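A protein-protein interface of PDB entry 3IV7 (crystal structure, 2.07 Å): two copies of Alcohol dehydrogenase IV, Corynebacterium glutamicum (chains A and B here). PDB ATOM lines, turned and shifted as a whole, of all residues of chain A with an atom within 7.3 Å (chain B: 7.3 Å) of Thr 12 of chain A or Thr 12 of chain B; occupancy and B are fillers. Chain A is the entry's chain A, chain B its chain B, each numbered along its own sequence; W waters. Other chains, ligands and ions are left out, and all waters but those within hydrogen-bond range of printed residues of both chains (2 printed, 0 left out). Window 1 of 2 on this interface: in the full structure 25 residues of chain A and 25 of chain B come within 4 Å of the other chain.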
ATOM      1  N   HIS A  10      30.388  19.095 -20.782  1.00  0.00           N
ATOM      2  CA  HIS A  10      29.394  18.172 -21.298  1.00  0.00           C
ATOM      3  C   HIS A  10      28.917  18.570 -22.699  1.00  0.00           C
ATOM      4  O   HIS A  10      28.513  19.721 -22.943  1.00  0.00           O
ATOM      5  CB  HIS A  10      28.194  18.088 -20.336  1.00  0.00           C
ATOM      6  CG  HIS A  10      27.087  17.220 -20.838  1.00  0.00           C
ATOM      7  ND1 HIS A  10      26.996  15.884 -20.528  1.00  0.00           N
ATOM      8  CD2 HIS A  10      26.075  17.475 -21.702  1.00  0.00           C
ATOM      9  CE1 HIS A  10      25.976  15.352 -21.177  1.00  0.00           C
ATOM     10  NE2 HIS A  10      25.392  16.302 -21.881  1.00  0.00           N
ATOM     11  N   ASP A  11      28.943  17.612 -23.603  1.00  0.00           N
ATOM     12  CA  ASP A  11      28.415  17.805 -24.948  1.00  0.00           C
ATOM     13  C   ASP A  11      27.057  17.149 -25.054  1.00  0.00           C
ATOM     14  O   ASP A  11      26.946  15.923 -25.002  1.00  0.00           O
ATOM     15  CB  ASP A  11      29.331  17.191 -25.983  1.00  0.00           C
ATOM     16  CG  ASP A  11      30.651  17.913 -26.077  1.00  0.00           C
ATOM     17  OD1 ASP A  11      30.668  19.085 -26.513  1.00  0.00           O
ATOM     18  OD2 ASP A  11      31.663  17.316 -25.710  1.00  0.00           O
ATOM     19  N   THR A  12      26.022  17.961 -25.206  1.00  0.00           N
ATOM     20  CA  THR A  12      24.708  17.426 -25.527  1.00  0.00           C
ATOM     21  C   THR A  12      24.629  17.349 -27.033  1.00  0.00           C
ATOM     22  O   THR A  12      24.779  18.341 -27.694  1.00  0.00           O
ATOM     23  CB  THR A  12      23.616  18.289 -25.005  1.00  0.00           C
ATOM     24  OG1 THR A  12      23.693  18.313 -23.569  1.00  0.00           O
ATOM     25  CG2 THR A  12      22.250  17.746 -25.460  1.00  0.00           C
ATOM     26  N   LEU A  13      24.408  16.145 -27.555  1.00  0.00           N
ATOM     27  CA  LEU A  13      24.408  15.906 -28.989  1.00  0.00           C
ATOM     28  C   LEU A  13      23.035  16.133 -29.584  1.00  0.00           C
ATOM     29  O   LEU A  13      22.038  15.758 -28.978  1.00  0.00           O
ATOM     30  CB  LEU A  13      24.838  14.467 -29.280  1.00  0.00           C
ATOM     31  CG  LEU A  13      26.221  14.079 -28.769  1.00  0.00           C
ATOM     32  CD1 LEU A  13      26.543  12.671 -29.193  1.00  0.00           C
ATOM     33  CD2 LEU A  13      27.326  15.081 -29.233  1.00  0.00           C
ATOM     34  N   PRO A  14      22.986  16.690 -30.814  1.00  0.00           N
ATOM     35  CA  PRO A  14      21.676  16.980 -31.427  1.00  0.00           C
ATOM     36  C   PRO A  14      20.990  15.713 -31.933  1.00  0.00           C
ATOM     37  O   PRO A  14      21.607  14.907 -32.600  1.00  0.00           O
ATOM     38  CB  PRO A  14      22.019  17.911 -32.587  1.00  0.00           C
ATOM     39  CG  PRO A  14      23.483  17.566 -32.943  1.00  0.00           C
ATOM     40  CD  PRO A  14      24.128  17.103 -31.665  1.00  0.00           C
ATOM     41  N   GLN A  15      19.742  15.523 -31.563  1.00  0.00           N
ATOM     42  CA  GLN A  15      18.991  14.390 -32.033  1.00  0.00           C
ATOM     43  C   GLN A  15      17.501  14.557 -31.824  1.00  0.00           C
ATOM     44  O   GLN A  15      17.058  15.141 -30.846  1.00  0.00           O
ATOM     45  CB  GLN A  15      19.457  13.110 -31.327  1.00  0.00           C
ATOM     46  CG  GLN A  15      19.202  11.852 -32.139  1.00  0.00           C
ATOM     47  CD  GLN A  15      19.943  10.644 -31.584  1.00  0.00           C
ATOM     48  OE1 GLN A  15      19.949  10.406 -30.371  1.00  0.00           O
ATOM     49  NE2 GLN A  15      20.568   9.868 -32.473  1.00  0.00           N
ATOM     50  N   LYS A  16      16.731  14.055 -32.782  1.00  0.00           N
ATOM     51  CA  LYS A  16      15.299  13.936 -32.643  1.00  0.00           C
ATOM     52  C   LYS A  16      14.972  12.464 -32.422  1.00  0.00           C
ATOM     53  O   LYS A  16      15.534  11.578 -33.092  1.00  0.00           O
ATOM     54  CB  LYS A  16      14.577  14.439 -33.887  1.00  0.00           C
ATOM     55  CG  LYS A  16      13.062  14.220 -33.868  1.00  0.00           C
ATOM     56  CD  LYS A  16      12.388  14.633 -35.231  1.00  0.00           C
ATOM     57  CE  LYS A  16      12.273  16.144 -35.389  1.00  0.00           C
ATOM     58  NZ  LYS A  16      11.375  16.765 -34.321  1.00  0.00           N
ATOM     59  N   VAL A  17      14.060  12.211 -31.504  1.00  0.00           N
ATOM     60  CA  VAL A  17      13.595  10.884 -31.207  1.00  0.00           C
ATOM     61  C   VAL A  17      12.110  10.866 -31.318  1.00  0.00           C
ATOM     62  O   VAL A  17      11.416  11.703 -30.700  1.00  0.00           O
ATOM     63  CB  VAL A  17      13.973  10.499 -29.766  1.00  0.00           C
ATOM     64  CG1 VAL A  17      13.585   9.029 -29.474  1.00  0.00           C
ATOM     65  CG2 VAL A  17      15.436  10.727 -29.553  1.00  0.00           C
ATOM     66  N   LEU A 145      31.014  13.000 -35.172  1.00  0.00           N
ATOM     67  CA  LEU A 145      29.618  13.539 -35.047  1.00  0.00           C
ATOM     68  C   LEU A 145      28.739  13.205 -36.255  1.00  0.00           C
ATOM     69  O   LEU A 145      27.535  13.037 -36.116  1.00  0.00           O
ATOM     70  CB  LEU A 145      29.613  15.062 -34.833  1.00  0.00           C
ATOM     71  CG  LEU A 145      28.197  15.723 -34.691  1.00  0.00           C
ATOM     72  CD1 LEU A 145      27.398  15.159 -33.443  1.00  0.00           C
ATOM     73  CD2 LEU A 145      28.290  17.290 -34.635  1.00  0.00           C
ATOM     74  N   LEU A 148      26.365  10.129 -35.924  1.00  0.00           N
ATOM     75  CA  LEU A 148      25.208  10.132 -35.038  1.00  0.00           C
ATOM     76  C   LEU A 148      23.937  10.289 -35.890  1.00  0.00           C
ATOM     77  O   LEU A 148      23.814  11.249 -36.615  1.00  0.00           O
ATOM     78  CB  LEU A 148      25.285  11.307 -34.043  1.00  0.00           C
ATOM     79  CG  LEU A 148      24.095  11.458 -33.087  1.00  0.00           C
ATOM     80  CD1 LEU A 148      24.056  10.277 -32.095  1.00  0.00           C
ATOM     81  CD2 LEU A 148      24.172  12.843 -32.345  1.00  0.00           C
ATOM     82  N   GLU A 150      20.615  11.600 -37.119  1.00  0.00           N
ATOM     83  CA  GLU A 150      19.915  12.833 -36.817  1.00  0.00           C
ATOM     84  C   GLU A 150      18.548  12.576 -36.222  1.00  0.00           C
ATOM     85  O   GLU A 150      18.049  13.375 -35.446  1.00  0.00           O
ATOM     86  CB  GLU A 150      19.766  13.671 -38.052  1.00  0.00           C
ATOM     87  CG  GLU A 150      21.018  14.277 -38.495  1.00  0.00           C
ATOM     88  CD  GLU A 150      20.831  15.240 -39.641  1.00  0.00           C
ATOM     89  OE1 GLU A 150      19.674  15.486 -40.055  1.00  0.00           O
ATOM     90  OE2 GLU A 150      21.850  15.726 -40.140  1.00  0.00           O
ATOM     91  N   ILE A 190      25.013  14.940 -15.679  1.00  0.00           N
ATOM     92  CA  ILE A 190      23.955  14.806 -16.673  1.00  0.00           C
ATOM     93  C   ILE A 190      23.947  13.397 -17.244  1.00  0.00           C
ATOM     94  O   ILE A 190      22.906  12.741 -17.245  1.00  0.00           O
ATOM     95  CB  ILE A 190      24.099  15.835 -17.794  1.00  0.00           C
ATOM     96  CG1 ILE A 190      23.975  17.238 -17.201  1.00  0.00           C
ATOM     97  CG2 ILE A 190      23.001  15.587 -18.904  1.00  0.00           C
ATOM     98  CD1 ILE A 190      24.543  18.333 -18.032  1.00  0.00           C
ATOM     99  N   LEU A 194      20.962  10.443 -16.696  1.00  0.00           N
ATOM    100  CA  LEU A 194      20.423   9.690 -17.840  1.00  0.00           C
ATOM    101  C   LEU A 194      20.705   8.185 -17.685  1.00  0.00           C
ATOM    102  O   LEU A 194      19.847   7.384 -17.947  1.00  0.00           O
ATOM    103  CB  LEU A 194      20.973  10.223 -19.173  1.00  0.00           C
ATOM    104  CG  LEU A 194      20.572  11.689 -19.482  1.00  0.00           C
ATOM    105  CD1 LEU A 194      21.195  12.172 -20.782  1.00  0.00           C
ATOM    106  CD2 LEU A 194      19.037  11.843 -19.525  1.00  0.00           C
ATOM    107  N   TYR A 227      17.689   3.802 -25.215  1.00  0.00           N
ATOM    108  CA  TYR A 227      18.044   5.111 -25.757  1.00  0.00           C
ATOM    109  C   TYR A 227      18.811   5.934 -24.732  1.00  0.00           C
ATOM    110  O   TYR A 227      19.925   6.433 -25.022  1.00  0.00           O
ATOM    111  CB  TYR A 227      16.814   5.874 -26.227  1.00  0.00           C
ATOM    112  CG  TYR A 227      17.177   7.222 -26.824  1.00  0.00           C
ATOM    113  CD1 TYR A 227      17.896   7.309 -28.001  1.00  0.00           C
ATOM    114  CD2 TYR A 227      16.837   8.403 -26.175  1.00  0.00           C
ATOM    115  CE1 TYR A 227      18.267   8.555 -28.535  1.00  0.00           C
ATOM    116  CE2 TYR A 227      17.171   9.636 -26.699  1.00  0.00           C
ATOM    117  CZ  TYR A 227      17.871   9.716 -27.879  1.00  0.00           C
ATOM    118  OH  TYR A 227      18.231  10.958 -28.360  1.00  0.00           O
ATOM    119  N   VAL A 231      22.686   7.385 -24.890  1.00  0.00           N
ATOM    120  CA  VAL A 231      22.939   8.818 -24.798  1.00  0.00           C
ATOM    121  C   VAL A 231      23.919   9.124 -23.636  1.00  0.00           C
ATOM    122  O   VAL A 231      24.836   9.946 -23.776  1.00  0.00           O
ATOM    123  CB  VAL A 231      21.638   9.621 -24.616  1.00  0.00           C
ATOM    124  CG1 VAL A 231      21.956  11.104 -24.301  1.00  0.00           C
ATOM    125  CG2 VAL A 231      20.726   9.527 -25.943  1.00  0.00           C
ATOM    126  N   SER A 235      28.160  10.245 -24.027  1.00  0.00           N
ATOM    127  CA  SER A 235      28.761  11.305 -23.248  1.00  0.00           C
ATOM    128  C   SER A 235      29.873  10.815 -22.309  1.00  0.00           C
ATOM    129  O   SER A 235      30.936  11.422 -22.240  1.00  0.00           O
ATOM    130  CB  SER A 235      27.700  12.034 -22.417  1.00  0.00           C
ATOM    131  OG  SER A 235      28.313  12.966 -21.507  1.00  0.00           O
ATOM    132  N   HIS B  10      10.693  13.869 -29.283  1.00  0.00           N
ATOM    133  CA  HIS B  10      11.589  14.722 -28.516  1.00  0.00           C
ATOM    134  C   HIS B  10      12.704  15.262 -29.379  1.00  0.00           C
ATOM    135  O   HIS B  10      13.263  14.520 -30.262  1.00  0.00           O
ATOM    136  CB  HIS B  10      12.190  13.945 -27.340  1.00  0.00           C
ATOM    137  CG  HIS B  10      13.046  14.785 -26.437  1.00  0.00           C
ATOM    138  ND1 HIS B  10      12.535  15.503 -25.394  1.00  0.00           N
ATOM    139  CD2 HIS B  10      14.380  15.034 -26.452  1.00  0.00           C
ATOM    140  CE1 HIS B  10      13.520  16.131 -24.772  1.00  0.00           C
ATOM    141  NE2 HIS B  10      14.649  15.872 -25.410  1.00  0.00           N
ATOM    142  N   ASP B  11      13.019  16.544 -29.168  1.00  0.00           N
ATOM    143  CA  ASP B  11      14.179  17.191 -29.819  1.00  0.00           C
ATOM    144  C   ASP B  11      15.179  17.543 -28.800  1.00  0.00           C
ATOM    145  O   ASP B  11      14.896  18.292 -27.902  1.00  0.00           O
ATOM    146  CB  ASP B  11      13.769  18.461 -30.585  1.00  0.00           C
ATOM    147  CG  ASP B  11      12.800  18.180 -31.670  1.00  0.00           C
ATOM    148  OD1 ASP B  11      13.055  17.272 -32.511  1.00  0.00           O
ATOM    149  OD2 ASP B  11      11.771  18.852 -31.698  1.00  0.00           O
ATOM    150  N   THR B  12      16.376  16.980 -28.926  1.00  0.00           N
ATOM    151  CA  THR B  12      17.452  17.313 -28.061  1.00  0.00           C
ATOM    152  C   THR B  12      18.331  18.298 -28.819  1.00  0.00           C
ATOM    153  O   THR B  12      18.772  18.027 -29.916  1.00  0.00           O
ATOM    154  CB  THR B  12      18.282  16.125 -27.676  1.00  0.00           C
ATOM    155  OG1 THR B  12      17.480  15.181 -26.956  1.00  0.00           O
ATOM    156  CG2 THR B  12      19.503  16.584 -26.783  1.00  0.00           C
ATOM    157  N   LEU B  13      18.549  19.443 -28.221  1.00  0.00           N
ATOM    158  CA  LEU B  13      19.252  20.532 -28.865  1.00  0.00           C
ATOM    159  C   LEU B  13      20.735  20.428 -28.618  1.00  0.00           C
ATOM    160  O   LEU B  13      21.141  20.105 -27.528  1.00  0.00           O
ATOM    161  CB  LEU B  13      18.743  21.869 -28.304  1.00  0.00           C
ATOM    162  CG  LEU B  13      17.231  22.131 -28.453  1.00  0.00           C
ATOM    163  CD1 LEU B  13      16.835  23.474 -27.791  1.00  0.00           C
ATOM    164  CD2 LEU B  13      16.805  22.114 -29.881  1.00  0.00           C
ATOM    165  N   PRO B  14      21.551  20.788 -29.619  1.00  0.00           N
ATOM    166  CA  PRO B  14      23.012  20.744 -29.469  1.00  0.00           C
ATOM    167  C   PRO B  14      23.520  21.852 -28.554  1.00  0.00           C
ATOM    168  O   PRO B  14      23.104  22.981 -28.694  1.00  0.00           O
ATOM    169  CB  PRO B  14      23.525  20.980 -30.897  1.00  0.00           C
ATOM    170  CG  PRO B  14      22.425  21.772 -31.586  1.00  0.00           C
ATOM    171  CD  PRO B  14      21.130  21.298 -30.948  1.00  0.00           C
ATOM    172  N   GLN B  15      24.393  21.517 -27.606  1.00  0.00           N
ATOM    173  CA  GLN B  15      25.023  22.538 -26.751  1.00  0.00           C
ATOM    174  C   GLN B  15      26.208  21.956 -26.000  1.00  0.00           C
ATOM    175  O   GLN B  15      26.216  20.768 -25.664  1.00  0.00           O
ATOM    176  CB  GLN B  15      24.015  23.082 -25.734  1.00  0.00           C
ATOM    177  CG  GLN B  15      24.356  24.389 -25.187  1.00  0.00           C
ATOM    178  CD  GLN B  15      23.171  25.055 -24.559  1.00  0.00           C
ATOM    179  OE1 GLN B  15      22.534  24.484 -23.691  1.00  0.00           O
ATOM    180  NE2 GLN B  15      22.863  26.300 -24.996  1.00  0.00           N
ATOM    181  N   LYS B  16      27.249  22.762 -25.834  1.00  0.00           N
ATOM    182  CA  LYS B  16      28.346  22.415 -24.972  1.00  0.00           C
ATOM    183  C   LYS B  16      28.153  23.169 -23.692  1.00  0.00           C
ATOM    184  O   LYS B  16      27.867  24.361 -23.721  1.00  0.00           O
ATOM    185  CB  LYS B  16      29.676  22.821 -25.579  1.00  0.00           C
ATOM    186  CG  LYS B  16      30.890  22.589 -24.638  1.00  0.00           C
ATOM    187  CD  LYS B  16      32.226  23.083 -25.237  1.00  0.00           C
ATOM    188  CE  LYS B  16      32.668  22.267 -26.442  1.00  0.00           C
ATOM    189  NZ  LYS B  16      32.700  20.784 -26.145  1.00  0.00           N
ATOM    190  N   VAL B  17      28.372  22.499 -22.569  1.00  0.00           N
ATOM    191  CA  VAL B  17      28.318  23.145 -21.259  1.00  0.00           C
ATOM    192  C   VAL B  17      29.611  22.936 -20.526  1.00  0.00           C
ATOM    193  O   VAL B  17      30.022  21.789 -20.301  1.00  0.00           O
ATOM    194  CB  VAL B  17      27.183  22.562 -20.411  1.00  0.00           C
ATOM    195  CG1 VAL B  17      27.112  23.257 -19.056  1.00  0.00           C
ATOM    196  CG2 VAL B  17      25.900  22.682 -21.150  1.00  0.00           C
ATOM    197  N   LEU B 145      17.004  27.765 -33.982  1.00  0.00           N
ATOM    198  CA  LEU B 145      18.248  27.132 -33.528  1.00  0.00           C
ATOM    199  C   LEU B 145      19.451  28.107 -33.552  1.00  0.00           C
ATOM    200  O   LEU B 145      20.371  27.965 -32.760  1.00  0.00           O
ATOM    201  CB  LEU B 145      18.563  25.900 -34.380  1.00  0.00           C
ATOM    202  CG  LEU B 145      19.827  25.106 -34.004  1.00  0.00           C
ATOM    203  CD1 LEU B 145      19.784  24.652 -32.532  1.00  0.00           C
ATOM    204  CD2 LEU B 145      20.015  23.908 -34.974  1.00  0.00           C
ATOM    205  N   LEU B 148      20.102  29.767 -30.054  1.00  0.00           N
ATOM    206  CA  LEU B 148      20.589  28.913 -28.970  1.00  0.00           C
ATOM    207  C   LEU B 148      22.110  29.047 -28.839  1.00  0.00           C
ATOM    208  O   LEU B 148      22.834  28.765 -29.795  1.00  0.00           O
ATOM    209  CB  LEU B 148      20.258  27.421 -29.286  1.00  0.00           C
ATOM    210  CG  LEU B 148      20.814  26.388 -28.294  1.00  0.00           C
ATOM    211  CD1 LEU B 148      20.125  26.539 -26.960  1.00  0.00           C
ATOM    212  CD2 LEU B 148      20.650  24.980 -28.841  1.00  0.00           C
ATOM    213  N   GLU B 150      25.797  28.096 -28.488  1.00  0.00           N
ATOM    214  CA  GLU B 150      26.479  26.876 -28.777  1.00  0.00           C
ATOM    215  C   GLU B 150      27.236  26.345 -27.580  1.00  0.00           C
ATOM    216  O   GLU B 150      27.387  25.124 -27.417  1.00  0.00           O
ATOM    217  CB  GLU B 150      27.427  27.064 -29.935  1.00  0.00           C
ATOM    218  CG  GLU B 150      26.744  27.174 -31.250  1.00  0.00           C
ATOM    219  CD  GLU B 150      27.730  27.257 -32.437  1.00  0.00           C
ATOM    220  OE1 GLU B 150      28.960  27.199 -32.218  1.00  0.00           O
ATOM    221  OE2 GLU B 150      27.255  27.366 -33.578  1.00  0.00           O
ATOM    222  N   ILE B 190      11.720  12.350 -21.219  1.00  0.00           N
ATOM    223  CA  ILE B 190      13.064  12.848 -21.162  1.00  0.00           C
ATOM    224  C   ILE B 190      13.086  14.253 -20.499  1.00  0.00           C
ATOM    225  O   ILE B 190      13.805  14.472 -19.535  1.00  0.00           O
ATOM    226  CB  ILE B 190      13.706  12.912 -22.523  1.00  0.00           C
ATOM    227  CG1 ILE B 190      13.763  11.480 -23.148  1.00  0.00           C
ATOM    228  CG2 ILE B 190      15.146  13.538 -22.381  1.00  0.00           C
ATOM    229  CD1 ILE B 190      14.331  11.419 -24.572  1.00  0.00           C
ATOM    230  N   LEU B 194      14.763  15.450 -16.645  1.00  0.00           N
ATOM    231  CA  LEU B 194      15.613  16.596 -16.550  1.00  0.00           C
ATOM    232  C   LEU B 194      14.991  17.671 -15.663  1.00  0.00           C
ATOM    233  O   LEU B 194      15.700  18.302 -14.887  1.00  0.00           O
ATOM    234  CB  LEU B 194      15.926  17.154 -17.913  1.00  0.00           C
ATOM    235  CG  LEU B 194      16.756  16.245 -18.845  1.00  0.00           C
ATOM    236  CD1 LEU B 194      17.008  16.983 -20.166  1.00  0.00           C
ATOM    237  CD2 LEU B 194      18.099  15.816 -18.202  1.00  0.00           C
ATOM    238  N   TYR B 227      20.209  25.172 -15.238  1.00  0.00           N
ATOM    239  CA  TYR B 227      20.486  24.694 -16.582  1.00  0.00           C
ATOM    240  C   TYR B 227      19.496  23.646 -17.013  1.00  0.00           C
ATOM    241  O   TYR B 227      18.880  23.760 -18.078  1.00  0.00           O
ATOM    242  CB  TYR B 227      21.881  24.119 -16.707  1.00  0.00           C
ATOM    243  CG  TYR B 227      22.151  23.620 -18.112  1.00  0.00           C
ATOM    244  CD1 TYR B 227      22.014  24.488 -19.204  1.00  0.00           C
ATOM    245  CD2 TYR B 227      22.531  22.336 -18.355  1.00  0.00           C
ATOM    246  CE1 TYR B 227      22.234  24.088 -20.460  1.00  0.00           C
ATOM    247  CE2 TYR B 227      22.776  21.904 -19.669  1.00  0.00           C
ATOM    248  CZ  TYR B 227      22.640  22.809 -20.710  1.00  0.00           C
ATOM    249  OH  TYR B 227      22.868  22.453 -22.017  1.00  0.00           O
ATOM    250  N   VAL B 231      16.666  23.524 -19.987  1.00  0.00           N
ATOM    251  CA  VAL B 231      16.730  22.543 -21.097  1.00  0.00           C
ATOM    252  C   VAL B 231      15.388  21.765 -21.172  1.00  0.00           C
ATOM    253  O   VAL B 231      14.865  21.470 -22.285  1.00  0.00           O
ATOM    254  CB  VAL B 231      17.917  21.546 -20.921  1.00  0.00           C
ATOM    255  CG1 VAL B 231      17.819  20.357 -21.944  1.00  0.00           C
ATOM    256  CG2 VAL B 231      19.318  22.286 -21.032  1.00  0.00           C
ATOM    257  N   SER B 235      12.236  22.073 -24.247  1.00  0.00           N
ATOM    258  CA  SER B 235      11.641  20.920 -24.864  1.00  0.00           C
ATOM    259  C   SER B 235      10.140  20.844 -24.543  1.00  0.00           C
ATOM    260  O   SER B 235       9.341  20.700 -25.428  1.00  0.00           O
ATOM    261  CB  SER B 235      12.337  19.655 -24.403  1.00  0.00           C
ATOM    262  OG  SER B 235      11.556  18.520 -24.711  1.00  0.00           O
HETATM  263  O   HOH W   1      21.798  20.020 -22.677  1.00  0.00           O
HETATM  264  O   HOH W   2      18.951  12.916 -26.497  1.00  0.00           O
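The backbone carbonyl oxygen (O) of Gln 15 of chain A is in hydrogen-bond range of the backbone NH (N) of Thr 12 of chain B.
The backbone NH (N) of His 10 of chain B sits at hydrogen-bond distance from the backbone carbonyl oxygen (O) of Val 17 of chain A.
N of Thr 12 of chain A lies within hydrogen-bond range of O of Gln 15 of chain B, 2.9 Å away.
The side-chain amino group (NZ) of Lys 16 of chain A is in salt-bridge range of the side-chain carboxylate (OD1) of Asp 11 of chain B (2.5 Å).
OD1 of Asp 11 of chain A lies within salt-bridge range of NZ of Lys 16 of chain B.
The backbone NH (N) of His 10 of chain A lies within hydrogen-bond range of the backbone carbonyl oxygen (O) of Val 17 of chain B, at 2.8 Å.
The backbone carbonyl oxygen (O) of Glu 150 of chain B is in hydrogen-bond range of the backbone NH (N) of Lys 16 of chain B (2.8 Å).
OG of Ser 235 of chain A lies within hydrogen-bond range of ND1 of His 10 of chain A (3.3 Å).
The side-chain hydroxyl (OG1) of Thr 12 of chain B lies close to a ring nitrogen (NE2) of His 10 of chain B (3.3 Å).
The backbone NH of Lys 16 of chain A lies within hydrogen-bond range of the backbone carbonyl oxygen of Glu 150 of chain A, at 3.0 Å.
OE1 of Gln 15 of chain A lies within hydrogen-bond range of OH of Tyr 227 of chain A (2.7 Å).
OG of Ser 235 of chain B lies close to ND1 of His 10 of chain B.
His 10 of chain A touches Gln 15 of chain B.
Asp 11 of chain A touches Gln 15 of chain B (CA to O, 3.8 Å).
CG2 of Thr 12 of chain A touches CG2 of Thr 12 of chain B (3.3 Å).
O of Leu 13 of chain B touches CG2 of Thr 12 of chain A (3.3 Å).
O of Thr 12 of chain A touches CA of Pro 14 of chain B, 3.5 Å away.
Leu 13 of chain A touches Thr 12 of chain B (O to CG2, 3.5 Å).
Pro 14 of chain A touches Thr 12 of chain B (CA to O, 3.4 Å).
Asp 11 of chain B touches Gln 15 of chain A.
O of His 10 of chain B touches CA of Lys 16 of chain A, at 3.2 Å.
Tyr 227 of chain A touches Ile 190 of chain B (CE2 to CD1, 3.97 Å).
Printed residues of chain B within 4 Å of His 10 of chain A: Gln 15, Lys 16 and Val 17.
Thr 12 of chain A touches just these residues of chain B: Thr 12, Leu 13, Pro 14 and Gln 15.
Of the printed residues of chain B, Val 17 of chain A touches His 10 (2.7 Å).
Printed residues of chain B within 4 Å of Tyr 227 of chain A: Ile 190 (3.97 Å).
Thr 12 of chain B touches four residues of chain A.
Tyr 227 of chain B touches none of the printed residues of chain A.
The nearest residue of chain B that does not touch Thr 12 of chain A is Tyr 227 of chain B (4.5 Å).
The nearest residue of chain A that does not touch Thr 12 of chain B is Tyr 227 of chain A (4.5 Å).
The nearest printed residue of chain A that does not touch Gln 15 of chain B is Leu 13 of chain A (5.3 Å).
Printed residues of chain A that touch a printed residue of chain B: His 10, Asp 11, Thr 12, Leu 13, Pro 14, Gln 15, Lys 16, Val 17 and Tyr 227.
Hydrophobic or aromatic side chains of chain A within 4 Å of the printed part of chain B: Pro 14 and Tyr 227.
Among the printed residues, 19 pairs touch across the chains.
Thr 12 of chain A touches its own counterpart, Thr 12 of chain B.
Thr 12 of chain A touches Leu 13 of chain B, and with the chains exchanged Leu 13 of chain A touches Thr 12 of chain B.
Thr 12 of chain A touches Pro 14 of chain B, and with the chains exchanged Pro 14 of chain A touches Thr 12 of chain B.
Tyr 227 of chain A touches Ile 190 of chain B, but with the chains exchanged Ile 190 of chain A does not touch Tyr 227 of chain B (4.3 Å).
Positions printed for both chains: 10, 11, 12, 13, 14, 15, 16, 17, 145, 148, 150, 190, 194, 227, 231 and 235.
Of the 19 pairs that touch across the chains among the printed residues, 18 have their exchanged pair printed and touching as well.
Water W1 lies within hydrogen-bond range of the side-chain hydroxyl of Thr 12 of chain A and the side-chain hydroxyl of Tyr 227 of chain B.
Water W2 lies within hydrogen-bond range of OG1 of Thr 12 of chain B (2.7 Å) and OH of Tyr 227 of chain A (2.8 Å).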
